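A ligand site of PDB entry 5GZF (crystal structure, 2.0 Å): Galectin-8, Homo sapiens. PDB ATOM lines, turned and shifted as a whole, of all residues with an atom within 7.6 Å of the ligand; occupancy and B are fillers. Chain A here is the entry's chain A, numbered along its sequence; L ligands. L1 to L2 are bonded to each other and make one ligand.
Val 80 touches the ligand. CE2 of Trp 89 touches C4 of LG2 L2, 3.5 Å away.
N of Arg 72 lies within hydrogen-bond range of O of Cys 78 (2.8 Å). The backbone carbonyl oxygen (O) of Asn 82 sits at hydrogen-bond distance from the backbone NH (N) of His 68. The side-chain amide nitrogen (ND2) of Asn 82 is in hydrogen-bond range of the backbone carbonyl oxygen (O) of Gly 90 (2.9 Å). The side-chain amide oxygen (OD1) of Asn 82 sits close to the backbone carbonyl oxygen (O) of Arg 91 (3.3 Å). A ring nitrogen (ND1) of His 68 sits at hydrogen-bond distance from the side-chain carboxylate (OD1) of Asp 52. The guanidinium group (NH1) of Arg 48 sits at hydrogen-bond distance from the side-chain amide oxygen (OD1) of Asn 70 (3.4 Å). The side-chain amide oxygen of Gln 50 lies within hydrogen-bond range of the guanidinium group of Arg 48 (2.8 Å). The backbone NH (N) of Asn 70 lies within hydrogen-bond range of the backbone carbonyl oxygen (O) of Val 80, at 2.9 Å.
NH1 of Arg 72 is in hydrogen-bond range of O3 of LIG L1 (2.5 Å). The side-chain carboxylate (OE2) of Glu 92 lies within hydrogen-bond range of an oxygen (O3) of LIG L1. ND2 of Asn 82 sits at hydrogen-bond distance from O5 of LG2 L2 (2.8 Å). A ring nitrogen (NE2) of His 68 sits at hydrogen-bond distance from an oxygen (O3) of LG2 L2, 2.8 Å away. The guanidinium group (NH2) of Arg 48 lies within hydrogen-bond range of an oxygen (O2) of LG2 L2 (3.1 Å). The side-chain amide oxygen of Asn 70 sits at hydrogen-bond distance from an oxygen (O3) of LG2 L2.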
ATOM      1  N   ARG A  48      -8.866 -24.951   9.795  1.00  0.00           N
ATOM      2  CA  ARG A  48      -7.861 -24.026   9.268  1.00  0.00           C
ATOM      3  C   ARG A  48      -8.243 -22.603   9.654  1.00  0.00           C
ATOM      4  O   ARG A  48      -9.392 -22.319  10.020  1.00  0.00           O
ATOM      5  CB  ARG A  48      -7.736 -24.157   7.751  1.00  0.00           C
ATOM      6  CG  ARG A  48      -9.068 -24.071   7.026  1.00  0.00           C
ATOM      7  CD  ARG A  48      -8.831 -24.017   5.539  1.00  0.00           C
ATOM      8  NE  ARG A  48      -8.598 -22.672   5.056  1.00  0.00           N
ATOM      9  CZ  ARG A  48      -8.147 -22.389   3.832  1.00  0.00           C
ATOM     10  NH1 ARG A  48      -7.874 -23.380   2.990  1.00  0.00           N
ATOM     11  NH2 ARG A  48      -7.975 -21.141   3.450  1.00  0.00           N
ATOM     12  N   PHE A  49      -7.263 -21.712   9.562  1.00  0.00           N
ATOM     13  CA  PHE A  49      -7.533 -20.280   9.524  1.00  0.00           C
ATOM     14  C   PHE A  49      -6.473 -19.627   8.653  1.00  0.00           C
ATOM     15  O   PHE A  49      -5.518 -20.281   8.208  1.00  0.00           O
ATOM     16  CB  PHE A  49      -7.574 -19.664  10.931  1.00  0.00           C
ATOM     17  CG  PHE A  49      -6.223 -19.484  11.578  1.00  0.00           C
ATOM     18  CD1 PHE A  49      -5.522 -18.288  11.434  1.00  0.00           C
ATOM     19  CD2 PHE A  49      -5.687 -20.493  12.366  1.00  0.00           C
ATOM     20  CE1 PHE A  49      -4.288 -18.117  12.046  1.00  0.00           C
ATOM     21  CE2 PHE A  49      -4.462 -20.323  12.980  1.00  0.00           C
ATOM     22  CZ  PHE A  49      -3.761 -19.145  12.826  1.00  0.00           C
ATOM     23  N   GLN A  50      -6.659 -18.339   8.371  1.00  0.00           N
ATOM     24  CA  GLN A  50      -5.727 -17.641   7.511  1.00  0.00           C
ATOM     25  C   GLN A  50      -5.586 -16.185   7.925  1.00  0.00           C
ATOM     26  O   GLN A  50      -6.537 -15.541   8.387  1.00  0.00           O
ATOM     27  CB  GLN A  50      -6.142 -17.719   6.052  1.00  0.00           C
ATOM     28  CG  GLN A  50      -7.419 -16.989   5.739  1.00  0.00           C
ATOM     29  CD  GLN A  50      -8.125 -17.619   4.569  1.00  0.00           C
ATOM     30  OE1 GLN A  50      -8.619 -18.734   4.672  1.00  0.00           O
ATOM     31  NE2 GLN A  50      -8.162 -16.908   3.440  1.00  0.00           N
ATOM     32  N   ASP A  52      -4.463 -12.922   5.813  1.00  0.00           N
ATOM     33  CA  ASP A  52      -4.257 -12.464   4.445  1.00  0.00           C
ATOM     34  C   ASP A  52      -3.820 -11.005   4.422  1.00  0.00           C
ATOM     35  O   ASP A  52      -4.527 -10.126   4.898  1.00  0.00           O
ATOM     36  CB  ASP A  52      -5.536 -12.649   3.613  1.00  0.00           C
ATOM     37  CG  ASP A  52      -5.897 -14.117   3.399  1.00  0.00           C
ATOM     38  OD1 ASP A  52      -5.018 -15.010   3.519  1.00  0.00           O
ATOM     39  OD2 ASP A  52      -7.075 -14.392   3.090  1.00  0.00           O
ATOM     40  N   ARG A  62     -12.755 -10.675  -5.829  1.00  0.00           N
ATOM     41  CA  ARG A  62     -12.013 -10.836  -4.588  1.00  0.00           C
ATOM     42  C   ARG A  62     -10.664 -10.140  -4.671  1.00  0.00           C
ATOM     43  O   ARG A  62      -9.911 -10.347  -5.624  1.00  0.00           O
ATOM     44  CB  ARG A  62     -11.834 -12.309  -4.269  1.00  0.00           C
ATOM     45  CG  ARG A  62     -11.070 -12.519  -3.002  1.00  0.00           C
ATOM     46  CD  ARG A  62     -10.995 -13.992  -2.692  1.00  0.00           C
ATOM     47  NE  ARG A  62     -10.118 -14.205  -1.549  1.00  0.00           N
ATOM     48  CZ  ARG A  62      -9.840 -15.400  -1.061  1.00  0.00           C
ATOM     49  NH1 ARG A  62     -10.366 -16.491  -1.620  1.00  0.00           N
ATOM     50  NH2 ARG A  62      -9.028 -15.497  -0.025  1.00  0.00           N
ATOM     51  N   HIS A  68      -0.881 -14.891   1.705  1.00  0.00           N
ATOM     52  CA  HIS A  68      -1.879 -15.770   2.314  1.00  0.00           C
ATOM     53  C   HIS A  68      -1.114 -16.695   3.257  1.00  0.00           C
ATOM     54  O   HIS A  68      -0.284 -17.487   2.800  1.00  0.00           O
ATOM     55  CB  HIS A  68      -2.618 -16.518   1.204  1.00  0.00           C
ATOM     56  CG  HIS A  68      -3.563 -17.583   1.660  1.00  0.00           C
ATOM     57  ND1 HIS A  68      -4.682 -17.332   2.424  1.00  0.00           N
ATOM     58  CD2 HIS A  68      -3.589 -18.910   1.372  1.00  0.00           C
ATOM     59  CE1 HIS A  68      -5.332 -18.466   2.625  1.00  0.00           C
ATOM     60  NE2 HIS A  68      -4.684 -19.443   2.014  1.00  0.00           N
ATOM     61  N   ASN A  70      -1.673 -19.523   5.946  1.00  0.00           N
ATOM     62  CA  ASN A  70      -2.833 -20.391   6.143  1.00  0.00           C
ATOM     63  C   ASN A  70      -2.486 -21.673   6.906  1.00  0.00           C
ATOM     64  O   ASN A  70      -2.197 -22.718   6.299  1.00  0.00           O
ATOM     65  CB  ASN A  70      -3.479 -20.683   4.774  1.00  0.00           C
ATOM     66  CG  ASN A  70      -4.585 -21.716   4.841  1.00  0.00           C
ATOM     67  OD1 ASN A  70      -4.708 -22.542   3.920  1.00  0.00           O
ATOM     68  ND2 ASN A  70      -5.371 -21.708   5.913  1.00  0.00           N
ATOM     69  N   ARG A  72      -3.237 -25.057   8.621  1.00  0.00           N
ATOM     70  CA  ARG A  72      -4.239 -26.112   8.496  1.00  0.00           C
ATOM     71  C   ARG A  72      -3.949 -27.193   9.528  1.00  0.00           C
ATOM     72  O   ARG A  72      -2.788 -27.474   9.855  1.00  0.00           O
ATOM     73  CB  ARG A  72      -4.220 -26.709   7.094  1.00  0.00           C
ATOM     74  CG  ARG A  72      -4.353 -25.677   5.983  1.00  0.00           C
ATOM     75  CD  ARG A  72      -4.343 -26.322   4.602  1.00  0.00           C
ATOM     76  NE  ARG A  72      -4.563 -25.320   3.555  1.00  0.00           N
ATOM     77  CZ  ARG A  72      -4.664 -25.598   2.269  1.00  0.00           C
ATOM     78  NH1 ARG A  72      -4.569 -26.854   1.850  1.00  0.00           N
ATOM     79  NH2 ARG A  72      -4.863 -24.614   1.395  1.00  0.00           N
ATOM     80  N   CYS A  78      -0.078 -28.268   8.750  1.00  0.00           N
ATOM     81  CA  CYS A  78       0.925 -27.590   7.930  1.00  0.00           C
ATOM     82  C   CYS A  78       0.533 -26.123   7.861  1.00  0.00           C
ATOM     83  O   CYS A  78      -0.509 -25.708   8.369  1.00  0.00           O
ATOM     84  CB  CYS A  78       1.034 -28.179   6.521  1.00  0.00           C
ATOM     85  SG  CYS A  78      -0.467 -27.943   5.524  1.00  0.00           S
ATOM     86  N   VAL A  80       0.135 -23.481   4.671  1.00  0.00           N
ATOM     87  CA  VAL A  80       0.201 -23.166   3.256  1.00  0.00           C
ATOM     88  C   VAL A  80       0.343 -21.644   3.119  1.00  0.00           C
ATOM     89  O   VAL A  80      -0.414 -20.894   3.734  1.00  0.00           O
ATOM     90  CB  VAL A  80      -1.043 -23.683   2.521  1.00  0.00           C
ATOM     91  CG1 VAL A  80      -1.009 -23.265   1.067  1.00  0.00           C
ATOM     92  CG2 VAL A  80      -1.125 -25.213   2.638  1.00  0.00           C
ATOM     93  N   CYS A  81       1.314 -21.204   2.326  1.00  0.00           N
ATOM     94  CA  CYS A  81       1.445 -19.812   1.954  1.00  0.00           C
ATOM     95  C   CYS A  81       1.319 -19.684   0.446  1.00  0.00           C
ATOM     96  O   CYS A  81       1.793 -20.544  -0.302  1.00  0.00           O
ATOM     97  CB  CYS A  81       2.777 -19.232   2.409  1.00  0.00           C
ATOM     98  SG  CYS A  81       2.960 -19.218   4.195  1.00  0.00           S
ATOM     99  N   ASN A  82       0.669 -18.611   0.017  1.00  0.00           N
ATOM    100  CA  ASN A  82       0.389 -18.443  -1.394  1.00  0.00           C
ATOM    101  C   ASN A  82      -0.002 -16.998  -1.665  1.00  0.00           C
ATOM    102  O   ASN A  82      -0.074 -16.172  -0.742  1.00  0.00           O
ATOM    103  CB  ASN A  82      -0.722 -19.413  -1.855  1.00  0.00           C
ATOM    104  CG  ASN A  82      -0.628 -19.751  -3.318  1.00  0.00           C
ATOM    105  OD1 ASN A  82       0.045 -19.072  -4.089  1.00  0.00           O
ATOM    106  ND2 ASN A  82      -1.338 -20.807  -3.716  1.00  0.00           N
ATOM    107  N   THR A  83      -0.217 -16.700  -2.936  1.00  0.00           N
ATOM    108  CA  THR A  83      -0.603 -15.380  -3.408  1.00  0.00           C
ATOM    109  C   THR A  83      -1.798 -15.551  -4.336  1.00  0.00           C
ATOM    110  O   THR A  83      -1.819 -16.474  -5.161  1.00  0.00           O
ATOM    111  CB  THR A  83       0.582 -14.708  -4.123  1.00  0.00           C
ATOM    112  OG1 THR A  83       1.583 -14.362  -3.154  1.00  0.00           O
ATOM    113  CG2 THR A  83       0.148 -13.448  -4.876  1.00  0.00           C
ATOM    114  N   LEU A  84      -2.796 -14.691  -4.152  1.00  0.00           N
ATOM    115  CA  LEU A  84      -4.007 -14.695  -4.969  1.00  0.00           C
ATOM    116  C   LEU A  84      -3.989 -13.459  -5.860  1.00  0.00           C
ATOM    117  O   LEU A  84      -3.876 -12.343  -5.361  1.00  0.00           O
ATOM    118  CB  LEU A  84      -5.275 -14.706  -4.105  1.00  0.00           C
ATOM    119  CG  LEU A  84      -6.634 -14.838  -4.816  1.00  0.00           C
ATOM    120  CD1 LEU A  84      -6.905 -16.273  -5.198  1.00  0.00           C
ATOM    121  CD2 LEU A  84      -7.767 -14.264  -3.971  1.00  0.00           C
ATOM    122  N   TRP A  89      -5.223 -18.633  -7.406  1.00  0.00           N
ATOM    123  CA  TRP A  89      -4.101 -18.925  -6.523  1.00  0.00           C
ATOM    124  C   TRP A  89      -2.858 -19.289  -7.322  1.00  0.00           C
ATOM    125  O   TRP A  89      -2.941 -19.919  -8.377  1.00  0.00           O
ATOM    126  CB  TRP A  89      -4.460 -20.072  -5.577  1.00  0.00           C
ATOM    127  CG  TRP A  89      -5.444 -19.654  -4.529  1.00  0.00           C
ATOM    128  CD1 TRP A  89      -6.752 -20.030  -4.416  1.00  0.00           C
ATOM    129  CD2 TRP A  89      -5.188 -18.763  -3.429  1.00  0.00           C
ATOM    130  NE1 TRP A  89      -7.325 -19.433  -3.321  1.00  0.00           N
ATOM    131  CE2 TRP A  89      -6.382 -18.660  -2.695  1.00  0.00           C
ATOM    132  CE3 TRP A  89      -4.064 -18.060  -3.005  1.00  0.00           C
ATOM    133  CZ2 TRP A  89      -6.485 -17.866  -1.560  1.00  0.00           C
ATOM    134  CZ3 TRP A  89      -4.165 -17.284  -1.880  1.00  0.00           C
ATOM    135  CH2 TRP A  89      -5.373 -17.181  -1.166  1.00  0.00           C
ATOM    136  N   GLY A  90      -1.703 -18.896  -6.800  1.00  0.00           N
ATOM    137  CA  GLY A  90      -0.417 -19.203  -7.414  1.00  0.00           C
ATOM    138  C   GLY A  90       0.166 -20.498  -6.906  1.00  0.00           C
ATOM    139  O   GLY A  90      -0.536 -21.386  -6.435  1.00  0.00           O
ATOM    140  N   ARG A  91       1.508 -20.581  -6.983  1.00  0.00           N
ATOM    141  CA  ARG A  91       2.266 -21.748  -6.541  1.00  0.00           C
ATOM    142  C   ARG A  91       2.295 -21.823  -5.014  1.00  0.00           C
ATOM    143  O   ARG A  91       2.746 -20.875  -4.353  1.00  0.00           O
ATOM    144  CB  ARG A  91       3.702 -21.673  -7.081  1.00  0.00           C
ATOM    145  CG  ARG A  91       4.548 -22.934  -6.867  1.00  0.00           C
ATOM    146  CD  ARG A  91       5.714 -22.730  -5.901  1.00  0.00           C
ATOM    147  NE  ARG A  91       6.326 -24.004  -5.566  1.00  0.00           N
ATOM    148  CZ  ARG A  91       7.277 -24.201  -4.644  1.00  0.00           C
ATOM    149  NH1 ARG A  91       7.783 -23.175  -3.954  1.00  0.00           N
ATOM    150  NH2 ARG A  91       7.727 -25.420  -4.437  1.00  0.00           N
ATOM    151  N   GLU A  92       1.859 -22.949  -4.449  1.00  0.00           N
ATOM    152  CA  GLU A  92       1.825 -23.099  -2.996  1.00  0.00           C
ATOM    153  C   GLU A  92       3.213 -23.299  -2.410  1.00  0.00           C
ATOM    154  O   GLU A  92       4.032 -24.050  -2.958  1.00  0.00           O
ATOM    155  CB  GLU A  92       0.939 -24.270  -2.592  1.00  0.00           C
ATOM    156  CG  GLU A  92      -0.528 -24.020  -2.754  1.00  0.00           C
ATOM    157  CD  GLU A  92      -1.362 -25.143  -2.170  1.00  0.00           C
ATOM    158  OE1 GLU A  92      -0.795 -26.221  -1.877  1.00  0.00           O
ATOM    159  OE2 GLU A  92      -2.579 -24.929  -1.968  1.00  0.00           O
ATOM    160  N   GLU A  93       3.479 -22.641  -1.267  1.00  0.00           N
ATOM    161  CA  GLU A  93       4.698 -22.868  -0.489  1.00  0.00           C
ATOM    162  C   GLU A  93       4.273 -23.489   0.842  1.00  0.00           C
ATOM    163  O   GLU A  93       3.734 -22.809   1.716  1.00  0.00           O
ATOM    164  CB  GLU A  93       5.482 -21.576  -0.293  1.00  0.00           C
ATOM    165  CG  GLU A  93       5.872 -20.903  -1.597  1.00  0.00           C
ATOM    166  CD  GLU A  93       6.763 -19.709  -1.401  1.00  0.00           C
ATOM    167  OE1 GLU A  93       7.429 -19.628  -0.345  1.00  0.00           O
ATOM    168  OE2 GLU A  93       6.822 -18.850  -2.317  1.00  0.00           O
ATOM    169  N   ILE A  94       4.488 -24.794   0.977  1.00  0.00           N
ATOM    170  CA  ILE A  94       3.970 -25.550   2.113  1.00  0.00           C
ATOM    171  C   ILE A  94       5.082 -25.767   3.124  1.00  0.00           C
ATOM    172  O   ILE A  94       6.159 -26.285   2.796  1.00  0.00           O
ATOM    173  CB  ILE A  94       3.367 -26.895   1.665  1.00  0.00           C
ATOM    174  CG1 ILE A  94       2.275 -26.646   0.621  1.00  0.00           C
ATOM    175  CG2 ILE A  94       2.770 -27.624   2.848  1.00  0.00           C
ATOM    176  CD1 ILE A  94       1.596 -27.922   0.148  1.00  0.00           C
HETATM  177  C1  LIG L   1      -4.288 -27.932  -2.410  1.00  0.00           C
HETATM  178  C2  LIG L   1      -5.172 -27.038  -1.634  1.00  0.00           C
HETATM  179  C3  LIG L   1      -5.928 -26.111  -2.461  1.00  0.00           C
HETATM  180  C4  LIG L   1      -6.592 -26.787  -3.608  1.00  0.00           C
HETATM  181  C5  LIG L   1      -6.784 -25.785  -4.733  1.00  0.00           C
HETATM  182  C6  LIG L   1      -5.169 -28.854  -3.231  1.00  0.00           C
HETATM  183  O1  LIG L   1      -4.405 -29.721  -3.843  1.00  0.00           O
HETATM  184  O2  LIG L   1      -3.454 -28.732  -1.555  1.00  0.00           O
HETATM  185  O3  LIG L   1      -4.363 -26.319  -0.628  1.00  0.00           O
HETATM  186  O4  LIG L   1      -6.947 -25.374  -1.587  1.00  0.00           O
HETATM  187  O5  LIG L   1      -5.854 -27.906  -4.227  1.00  0.00           O
HETATM  188  O6  LIG L   1      -8.071 -25.255  -4.604  1.00  0.00           O
HETATM  189  C1  LG2 L   2      -6.835 -23.980  -1.647  1.00  0.00           C
HETATM  190  C2  LG2 L   2      -7.903 -23.288  -0.799  1.00  0.00           C
HETATM  191  C3  LG2 L   2      -7.769 -21.814  -0.655  1.00  0.00           C
HETATM  192  C4  LG2 L   2      -6.373 -21.360  -0.417  1.00  0.00           C
HETATM  193  C5  LG2 L   2      -5.367 -22.051  -1.331  1.00  0.00           C
HETATM  194  C6  LG2 L   2      -3.946 -21.713  -0.989  1.00  0.00           C
HETATM  195  O1  LG2 L   2      -9.251 -23.608  -1.244  1.00  0.00           O
HETATM  196  O2  LG2 L   2      -8.602 -21.439   0.460  1.00  0.00           O
HETATM  197  O3  LG2 L   2      -6.053 -21.692   0.962  1.00  0.00           O
HETATM  198  O4  LG2 L   2      -5.499 -23.525  -1.276  1.00  0.00           O
HETATM  199  O5  LG2 L   2      -3.141 -22.182  -2.045  1.00  0.00           O
